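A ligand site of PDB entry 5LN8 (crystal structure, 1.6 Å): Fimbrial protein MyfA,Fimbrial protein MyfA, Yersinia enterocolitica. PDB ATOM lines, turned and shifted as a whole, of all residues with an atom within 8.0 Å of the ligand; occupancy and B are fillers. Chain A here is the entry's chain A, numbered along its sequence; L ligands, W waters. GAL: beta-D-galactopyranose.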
ATOM      1  N   LYS A  35     -20.943  26.964  -1.837  1.00  0.00           N
ATOM      2  CA  LYS A  35     -22.325  26.765  -2.249  1.00  0.00           C
ATOM      3  C   LYS A  35     -22.830  25.368  -1.903  1.00  0.00           C
ATOM      4  O   LYS A  35     -23.967  25.203  -1.458  1.00  0.00           O
ATOM      5  CB  LYS A  35     -22.494  27.033  -3.750  1.00  0.00           C
ATOM      6  CG  LYS A  35     -23.938  27.012  -4.213  1.00  0.00           C
ATOM      7  CD  LYS A  35     -24.072  27.082  -5.720  1.00  0.00           C
ATOM      8  CE  LYS A  35     -25.538  26.978  -6.123  1.00  0.00           C
ATOM      9  NZ  LYS A  35     -25.727  27.038  -7.582  1.00  0.00           N
ATOM     10  N   GLY A  36     -21.990  24.361  -2.105  1.00  0.00           N
ATOM     11  CA  GLY A  36     -22.404  22.991  -1.865  1.00  0.00           C
ATOM     12  C   GLY A  36     -21.330  21.954  -2.132  1.00  0.00           C
ATOM     13  O   GLY A  36     -20.141  22.289  -2.175  1.00  0.00           O
ATOM     14  N   TRP A  37     -21.757  20.712  -2.339  1.00  0.00           N
ATOM     15  CA  TRP A  37     -20.853  19.573  -2.469  1.00  0.00           C
ATOM     16  C   TRP A  37     -21.268  18.600  -3.557  1.00  0.00           C
ATOM     17  O   TRP A  37     -22.455  18.442  -3.847  1.00  0.00           O
ATOM     18  CB  TRP A  37     -20.793  18.790  -1.146  1.00  0.00           C
ATOM     19  CG  TRP A  37     -20.523  19.601   0.077  1.00  0.00           C
ATOM     20  CD1 TRP A  37     -21.450  20.234   0.854  1.00  0.00           C
ATOM     21  CD2 TRP A  37     -19.255  19.845   0.696  1.00  0.00           C
ATOM     22  NE1 TRP A  37     -20.839  20.868   1.903  1.00  0.00           N
ATOM     23  CE2 TRP A  37     -19.483  20.641   1.836  1.00  0.00           C
ATOM     24  CE3 TRP A  37     -17.942  19.467   0.382  1.00  0.00           C
ATOM     25  CZ2 TRP A  37     -18.448  21.070   2.664  1.00  0.00           C
ATOM     26  CZ3 TRP A  37     -16.928  19.892   1.216  1.00  0.00           C
ATOM     27  CH2 TRP A  37     -17.185  20.688   2.340  1.00  0.00           C
ATOM     28  N   ASN A  38     -20.278  17.935  -4.147  1.00  0.00           N
ATOM     29  CA  ASN A  38     -20.516  16.771  -4.989  1.00  0.00           C
ATOM     30  C   ASN A  38     -19.906  15.551  -4.312  1.00  0.00           C
ATOM     31  O   ASN A  38     -18.908  15.662  -3.592  1.00  0.00           O
ATOM     32  CB  ASN A  38     -19.867  16.927  -6.383  1.00  0.00           C
ATOM     33  CG  ASN A  38     -20.515  18.013  -7.230  1.00  0.00           C
ATOM     34  OD1 ASN A  38     -21.737  18.179  -7.267  1.00  0.00           O
ATOM     35  ND2 ASN A  38     -19.672  18.741  -7.960  1.00  0.00           N
ATOM     36  N   VAL A  39     -20.497  14.387  -4.534  1.00  0.00           N
ATOM     37  CA  VAL A  39     -19.862  13.126  -4.200  1.00  0.00           C
ATOM     38  C   VAL A  39     -19.891  12.274  -5.457  1.00  0.00           C
ATOM     39  O   VAL A  39     -20.942  11.735  -5.827  1.00  0.00           O
ATOM     40  CB  VAL A  39     -20.578  12.398  -3.060  1.00  0.00           C
ATOM     41  CG1 VAL A  39     -19.824  11.136  -2.711  1.00  0.00           C
ATOM     42  CG2 VAL A  39     -20.723  13.305  -1.837  1.00  0.00           C
ATOM     43  N   ARG A  40     -18.746  12.186  -6.131  1.00  0.00           N
ATOM     44  CA  ARG A  40     -18.646  11.511  -7.426  1.00  0.00           C
ATOM     45  C   ARG A  40     -18.038  10.121  -7.268  1.00  0.00           C
ATOM     46  O   ARG A  40     -16.895  10.000  -6.843  1.00  0.00           O
ATOM     47  CB  ARG A  40     -17.815  12.334  -8.413  1.00  0.00           C
ATOM     48  CG  ARG A  40     -18.380  13.727  -8.725  1.00  0.00           C
ATOM     49  CD  ARG A  40     -17.648  14.378  -9.895  1.00  0.00           C
ATOM     50  NE  ARG A  40     -18.183  15.686 -10.293  1.00  0.00           N
ATOM     51  CZ  ARG A  40     -19.222  15.854 -11.097  1.00  0.00           C
ATOM     52  NH1 ARG A  40     -19.861  14.809 -11.590  1.00  0.00           N
ATOM     53  NH2 ARG A  40     -19.639  17.067 -11.424  1.00  0.00           N
ATOM     54  N   SER A  66     -28.908  14.777  -2.940  1.00  0.00           N
ATOM     55  CA  SER A  66     -29.597  14.570  -4.219  1.00  0.00           C
ATOM     56  C   SER A  66     -28.699  13.781  -5.170  1.00  0.00           C
ATOM     57  O   SER A  66     -27.518  13.600  -4.898  1.00  0.00           O
ATOM     58  CB  SER A  66     -29.967  15.905  -4.888  1.00  0.00           C
ATOM     59  OG  SER A  66     -30.701  16.753  -4.034  1.00  0.00           O
ATOM     60  N   TRP A  67     -29.266  13.360  -6.303  1.00  0.00           N
ATOM     61  CA  TRP A  67     -28.522  12.608  -7.298  1.00  0.00           C
ATOM     62  C   TRP A  67     -28.773  13.222  -8.675  1.00  0.00           C
ATOM     63  O   TRP A  67     -29.883  13.636  -8.975  1.00  0.00           O
ATOM     64  CB  TRP A  67     -28.967  11.142  -7.261  1.00  0.00           C
ATOM     65  CG  TRP A  67     -28.388  10.273  -8.331  1.00  0.00           C
ATOM     66  CD1 TRP A  67     -28.948   9.986  -9.539  1.00  0.00           C
ATOM     67  CD2 TRP A  67     -27.155   9.536  -8.271  1.00  0.00           C
ATOM     68  NE1 TRP A  67     -28.137   9.122 -10.243  1.00  0.00           N
ATOM     69  CE2 TRP A  67     -27.034   8.834  -9.482  1.00  0.00           C
ATOM     70  CE3 TRP A  67     -26.135   9.418  -7.318  1.00  0.00           C
ATOM     71  CZ2 TRP A  67     -25.930   8.013  -9.770  1.00  0.00           C
ATOM     72  CZ3 TRP A  67     -25.050   8.615  -7.596  1.00  0.00           C
ATOM     73  CH2 TRP A  67     -24.948   7.920  -8.816  1.00  0.00           C
ATOM     74  N   ASP A  68     -27.716  13.288  -9.484  1.00  0.00           N
ATOM     75  CA  ASP A  68     -27.794  13.826 -10.831  1.00  0.00           C
ATOM     76  C   ASP A  68     -27.068  12.892 -11.803  1.00  0.00           C
ATOM     77  O   ASP A  68     -25.854  13.010 -12.007  1.00  0.00           O
ATOM     78  CB  ASP A  68     -27.192  15.224 -10.884  1.00  0.00           C
ATOM     79  CG  ASP A  68     -27.320  15.886 -12.244  1.00  0.00           C
ATOM     80  OD1 ASP A  68     -27.965  15.338 -13.157  1.00  0.00           O
ATOM     81  OD2 ASP A  68     -26.784  16.998 -12.398  1.00  0.00           O
ATOM     82  N   ASN A  69     -27.831  11.960 -12.391  1.00  0.00           N
ATOM     83  CA  ASN A  69     -27.324  11.022 -13.385  1.00  0.00           C
ATOM     84  C   ASN A  69     -26.255  10.065 -12.884  1.00  0.00           C
ATOM     85  O   ASN A  69     -26.415   8.853 -13.005  1.00  0.00           O
ATOM     86  CB  ASN A  69     -26.812  11.739 -14.637  1.00  0.00           C
ATOM     87  CG  ASN A  69     -27.924  12.080 -15.599  1.00  0.00           C
ATOM     88  OD1 ASN A  69     -28.837  11.291 -15.810  1.00  0.00           O
ATOM     89  ND2 ASN A  69     -27.839  13.267 -16.202  1.00  0.00           N
ATOM     90  N   ASP A  70     -25.179  10.605 -12.333  1.00  0.00           N
ATOM     91  CA  ASP A  70     -24.038   9.774 -11.967  1.00  0.00           C
ATOM     92  C   ASP A  70     -23.310  10.204 -10.702  1.00  0.00           C
ATOM     93  O   ASP A  70     -22.189   9.761 -10.448  1.00  0.00           O
ATOM     94  CB  ASP A  70     -23.031   9.750 -13.117  1.00  0.00           C
ATOM     95  CG  ASP A  70     -22.600  11.134 -13.559  1.00  0.00           C
ATOM     96  OD1 ASP A  70     -22.774  12.104 -12.797  1.00  0.00           O
ATOM     97  OD2 ASP A  70     -22.077  11.251 -14.684  1.00  0.00           O
ATOM     98  N   HIS A  71     -23.927  11.075  -9.914  1.00  0.00           N
ATOM     99  CA  HIS A  71     -23.257  11.581  -8.715  1.00  0.00           C
ATOM    100  C   HIS A  71     -24.233  12.204  -7.724  1.00  0.00           C
ATOM    101  O   HIS A  71     -25.300  12.673  -8.114  1.00  0.00           O
ATOM    102  CB  HIS A  71     -22.176  12.596  -9.103  1.00  0.00           C
ATOM    103  CG  HIS A  71     -22.712  13.893  -9.636  1.00  0.00           C
ATOM    104  ND1 HIS A  71     -23.139  14.041 -10.924  1.00  0.00           N
ATOM    105  CD2 HIS A  71     -22.851  15.109  -9.049  1.00  0.00           C
ATOM    106  CE1 HIS A  71     -23.544  15.284 -11.125  1.00  0.00           C
ATOM    107  NE2 HIS A  71     -23.379  15.956  -9.998  1.00  0.00           N
ATOM    108  N   TRP A  72     -23.886  12.169  -6.450  1.00  0.00           N
ATOM    109  CA  TRP A  72     -24.665  12.870  -5.435  1.00  0.00           C
ATOM    110  C   TRP A  72     -24.200  14.336  -5.342  1.00  0.00           C
ATOM    111  O   TRP A  72     -23.067  14.656  -5.709  1.00  0.00           O
ATOM    112  CB  TRP A  72     -24.611  12.180  -4.069  1.00  0.00           C
ATOM    113  CG  TRP A  72     -25.208  10.795  -4.068  1.00  0.00           C
ATOM    114  CD1 TRP A  72     -26.522  10.467  -3.949  1.00  0.00           C
ATOM    115  CD2 TRP A  72     -24.494   9.553  -4.189  1.00  0.00           C
ATOM    116  NE1 TRP A  72     -26.680   9.106  -4.006  1.00  0.00           N
ATOM    117  CE2 TRP A  72     -25.448   8.522  -4.147  1.00  0.00           C
ATOM    118  CE3 TRP A  72     -23.151   9.223  -4.335  1.00  0.00           C
ATOM    119  CZ2 TRP A  72     -25.097   7.180  -4.244  1.00  0.00           C
ATOM    120  CZ3 TRP A  72     -22.800   7.889  -4.426  1.00  0.00           C
ATOM    121  CH2 TRP A  72     -23.771   6.881  -4.382  1.00  0.00           C
ATOM    122  N   TRP A  73     -25.101  15.202  -4.903  1.00  0.00           N
ATOM    123  CA  TRP A  73     -24.815  16.636  -4.747  1.00  0.00           C
ATOM    124  C   TRP A  73     -25.789  17.257  -3.770  1.00  0.00           C
ATOM    125  O   TRP A  73     -26.864  16.689  -3.508  1.00  0.00           O
ATOM    126  CB  TRP A  73     -24.868  17.372  -6.091  1.00  0.00           C
ATOM    127  CG  TRP A  73     -26.261  17.481  -6.675  1.00  0.00           C
ATOM    128  CD1 TRP A  73     -26.925  16.530  -7.390  1.00  0.00           C
ATOM    129  CD2 TRP A  73     -27.140  18.609  -6.614  1.00  0.00           C
ATOM    130  NE1 TRP A  73     -28.157  16.983  -7.754  1.00  0.00           N
ATOM    131  CE2 TRP A  73     -28.311  18.269  -7.292  1.00  0.00           C
ATOM    132  CE3 TRP A  73     -27.032  19.879  -6.039  1.00  0.00           C
ATOM    133  CZ2 TRP A  73     -29.386  19.146  -7.425  1.00  0.00           C
ATOM    134  CZ3 TRP A  73     -28.108  20.750  -6.164  1.00  0.00           C
ATOM    135  CH2 TRP A  73     -29.259  20.385  -6.858  1.00  0.00           C
ATOM    136  N   ILE A  74     -25.416  18.411  -3.232  1.00  0.00           N
ATOM    137  CA  ILE A  74     -26.308  19.187  -2.379  1.00  0.00           C
ATOM    138  C   ILE A  74     -25.832  20.627  -2.317  1.00  0.00           C
ATOM    139  O   ILE A  74     -24.629  20.882  -2.255  1.00  0.00           O
ATOM    140  CB  ILE A  74     -26.412  18.584  -0.957  1.00  0.00           C
ATOM    141  CG1 ILE A  74     -27.476  19.308  -0.130  1.00  0.00           C
ATOM    142  CG2 ILE A  74     -25.067  18.602  -0.258  1.00  0.00           C
ATOM    143  CD1 ILE A  74     -27.699  18.672   1.239  1.00  0.00           C
ATOM    144  N   ASP A  75     -26.766  21.571  -2.392  1.00  0.00           N
ATOM    145  CA  ASP A  75     -26.448  22.938  -2.067  1.00  0.00           C
ATOM    146  C   ASP A  75     -26.588  23.087  -0.558  1.00  0.00           C
ATOM    147  O   ASP A  75     -27.681  22.953  -0.007  1.00  0.00           O
ATOM    148  CB  ASP A  75     -27.400  23.883  -2.787  1.00  0.00           C
ATOM    149  CG  ASP A  75     -27.155  23.929  -4.272  1.00  0.00           C
ATOM    150  OD1 ASP A  75     -26.065  23.541  -4.700  1.00  0.00           O
ATOM    151  OD2 ASP A  75     -28.065  24.381  -5.006  1.00  0.00           O
ATOM    152  N   GLU A 105     -16.260  16.808  -3.682  1.00  0.00           N
ATOM    153  CA  GLU A 105     -15.918  18.114  -4.234  1.00  0.00           C
ATOM    154  C   GLU A 105     -16.707  19.223  -3.556  1.00  0.00           C
ATOM    155  O   GLU A 105     -17.907  19.073  -3.311  1.00  0.00           O
ATOM    156  CB  GLU A 105     -16.165  18.159  -5.739  1.00  0.00           C
ATOM    157  CG  GLU A 105     -15.364  17.158  -6.574  1.00  0.00           C
ATOM    158  CD  GLU A 105     -15.790  17.139  -8.039  1.00  0.00           C
ATOM    159  OE1 GLU A 105     -16.930  17.539  -8.353  1.00  0.00           O
ATOM    160  OE2 GLU A 105     -14.991  16.723  -8.885  1.00  0.00           O
ATOM    161  N   TYR A 107     -17.906  23.136  -4.055  1.00  0.00           N
ATOM    162  CA  TYR A 107     -18.041  24.133  -5.112  1.00  0.00           C
ATOM    163  C   TYR A 107     -18.636  25.454  -4.636  1.00  0.00           C
ATOM    164  O   TYR A 107     -19.290  25.511  -3.588  1.00  0.00           O
ATOM    165  CB  TYR A 107     -18.827  23.576  -6.292  1.00  0.00           C
ATOM    166  CG  TYR A 107     -20.230  23.103  -5.980  1.00  0.00           C
ATOM    167  CD1 TYR A 107     -21.277  23.995  -5.819  1.00  0.00           C
ATOM    168  CD2 TYR A 107     -20.519  21.745  -5.889  1.00  0.00           C
ATOM    169  CE1 TYR A 107     -22.562  23.563  -5.548  1.00  0.00           C
ATOM    170  CE2 TYR A 107     -21.796  21.306  -5.609  1.00  0.00           C
ATOM    171  CZ  TYR A 107     -22.812  22.217  -5.442  1.00  0.00           C
ATOM    172  OH  TYR A 107     -24.089  21.762  -5.174  1.00  0.00           O
ATOM    173  N   VAL A 108     -18.386  26.519  -5.397  1.00  0.00           N
ATOM    174  CA  VAL A 108     -18.925  27.839  -5.117  1.00  0.00           C
ATOM    175  C   VAL A 108     -19.657  28.390  -6.333  1.00  0.00           C
ATOM    176  O   VAL A 108     -19.353  28.039  -7.465  1.00  0.00           O
ATOM    177  CB  VAL A 108     -17.831  28.841  -4.680  1.00  0.00           C
ATOM    178  CG1 VAL A 108     -17.156  28.365  -3.429  1.00  0.00           C
ATOM    179  CG2 VAL A 108     -16.797  29.063  -5.791  1.00  0.00           C
ATOM    180  N   PRO A 115     -20.505  25.674 -11.674  1.00  0.00           N
ATOM    181  CA  PRO A 115     -19.901  26.251 -10.467  1.00  0.00           C
ATOM    182  C   PRO A 115     -18.461  25.796 -10.304  1.00  0.00           C
ATOM    183  O   PRO A 115     -18.087  24.731 -10.781  1.00  0.00           O
ATOM    184  CB  PRO A 115     -20.745  25.664  -9.328  1.00  0.00           C
ATOM    185  CG  PRO A 115     -21.826  24.861  -9.978  1.00  0.00           C
ATOM    186  CD  PRO A 115     -21.359  24.528 -11.352  1.00  0.00           C
ATOM    187  N   THR A 116     -17.655  26.599  -9.630  1.00  0.00           N
ATOM    188  CA  THR A 116     -16.238  26.310  -9.520  1.00  0.00           C
ATOM    189  C   THR A 116     -15.966  25.371  -8.361  1.00  0.00           C
ATOM    190  O   THR A 116     -16.439  25.605  -7.253  1.00  0.00           O
ATOM    191  CB  THR A 116     -15.455  27.599  -9.301  1.00  0.00           C
ATOM    192  OG1 THR A 116     -15.707  28.495 -10.388  1.00  0.00           O
ATOM    193  CG2 THR A 116     -13.966  27.315  -9.215  1.00  0.00           C
ATOM    194  N   VAL A 117     -15.218  24.294  -8.617  1.00  0.00           N
ATOM    195  CA  VAL A 117     -14.772  23.420  -7.548  1.00  0.00           C
ATOM    196  C   VAL A 117     -13.537  24.014  -6.908  1.00  0.00           C
ATOM    197  O   VAL A 117     -12.552  24.304  -7.596  1.00  0.00           O
ATOM    198  CB  VAL A 117     -14.453  22.019  -8.061  1.00  0.00           C
ATOM    199  CG1 VAL A 117     -13.846  21.178  -6.957  1.00  0.00           C
ATOM    200  CG2 VAL A 117     -15.714  21.360  -8.565  1.00  0.00           C
HETATM  201  C1  GAL L   1     -26.543  20.701  -9.755  1.00  0.00           C
HETATM  202  C2  GAL L   1     -25.362  19.739 -10.026  1.00  0.00           C
HETATM  203  C3  GAL L   1     -24.340  19.825  -8.879  1.00  0.00           C
HETATM  204  C4  GAL L   1     -23.862  21.278  -8.719  1.00  0.00           C
HETATM  205  C5  GAL L   1     -25.072  22.229  -8.599  1.00  0.00           C
HETATM  206  C6  GAL L   1     -24.704  23.721  -8.652  1.00  0.00           C
HETATM  207  O1  GAL L   1     -27.468  20.686 -10.783  1.00  0.00           O
HETATM  208  O2  GAL L   1     -25.763  18.364 -10.191  1.00  0.00           O
HETATM  209  O3  GAL L   1     -23.202  19.003  -9.100  1.00  0.00           O
HETATM  210  O4  GAL L   1     -23.026  21.686  -9.805  1.00  0.00           O
HETATM  211  O5  GAL L   1     -26.050  22.030  -9.648  1.00  0.00           O
HETATM  212  O6  GAL L   1     -25.804  24.560  -8.388  1.00  0.00           O
HETATM  213  O   HOH W   1     -20.374  20.808  -9.878  1.00  0.00           O
HETATM  214  O   HOH W   2     -22.154  18.589 -12.019  1.00  0.00           O
HETATM  215  O   HOH W   3     -25.892  25.992 -11.205  1.00  0.00           O
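NE2 of His 71 sits at hydrogen-bond distance from O3 of the ligand (3.2 Å).
The side-chain carboxylate (OD2) of Asp 68 lies within hydrogen-bond range of an oxygen (O2) of the ligand (2.8 Å).
The side-chain amino group (NZ) of Lys 35 sits at hydrogen-bond distance from an oxygen (O6) of the ligand.
OD1 of Asn 38 is in hydrogen-bond range of O3 of the ligand.
The side-chain carboxylate of Asp 70 lies within hydrogen-bond range of a ring nitrogen (ND1) of His 71 (2.7 Å).
O of Trp 73 sits at hydrogen-bond distance from N of Ser 66 (2.9 Å).
The backbone NH of Asn 38 lies within hydrogen-bond range of the backbone carbonyl oxygen of Glu 105, 2.8 Å away.
OH of Tyr 107 sits at hydrogen-bond distance from OD1 of Asp 75 (2.7 Å).
A ring nitrogen (ND1) of His 71 sits at hydrogen-bond distance from the guanidinium group of Arg 40 (3.4 Å).
OH of Tyr 107 sits at hydrogen-bond distance from O of Ile 74.
O of Tyr 107 lies within hydrogen-bond range of N of Lys 35 (2.8 Å).
The backbone carbonyl oxygen (O) of Asp 68 lies within hydrogen-bond range of a ring nitrogen (ND1) of His 71 (3.1 Å).
Residues that only touch the ligand: Trp 73 (3.5 Å), Asp 75 (3.8 Å), Tyr 107 (3.6 Å) and Pro 115 (3.4 Å).
Hydrophobic or aromatic side chains that line the ligand: His 71, Trp 73, Tyr 107 and Pro 115.
Water W1 lies within hydrogen-bond range of O4 of the ligand and ND2 of Asn 38.
Water W2 bridges the guanidinium group (NH2) of Arg 40 (3.0 Å) and an oxygen (O3) of the ligand (3.1 Å).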
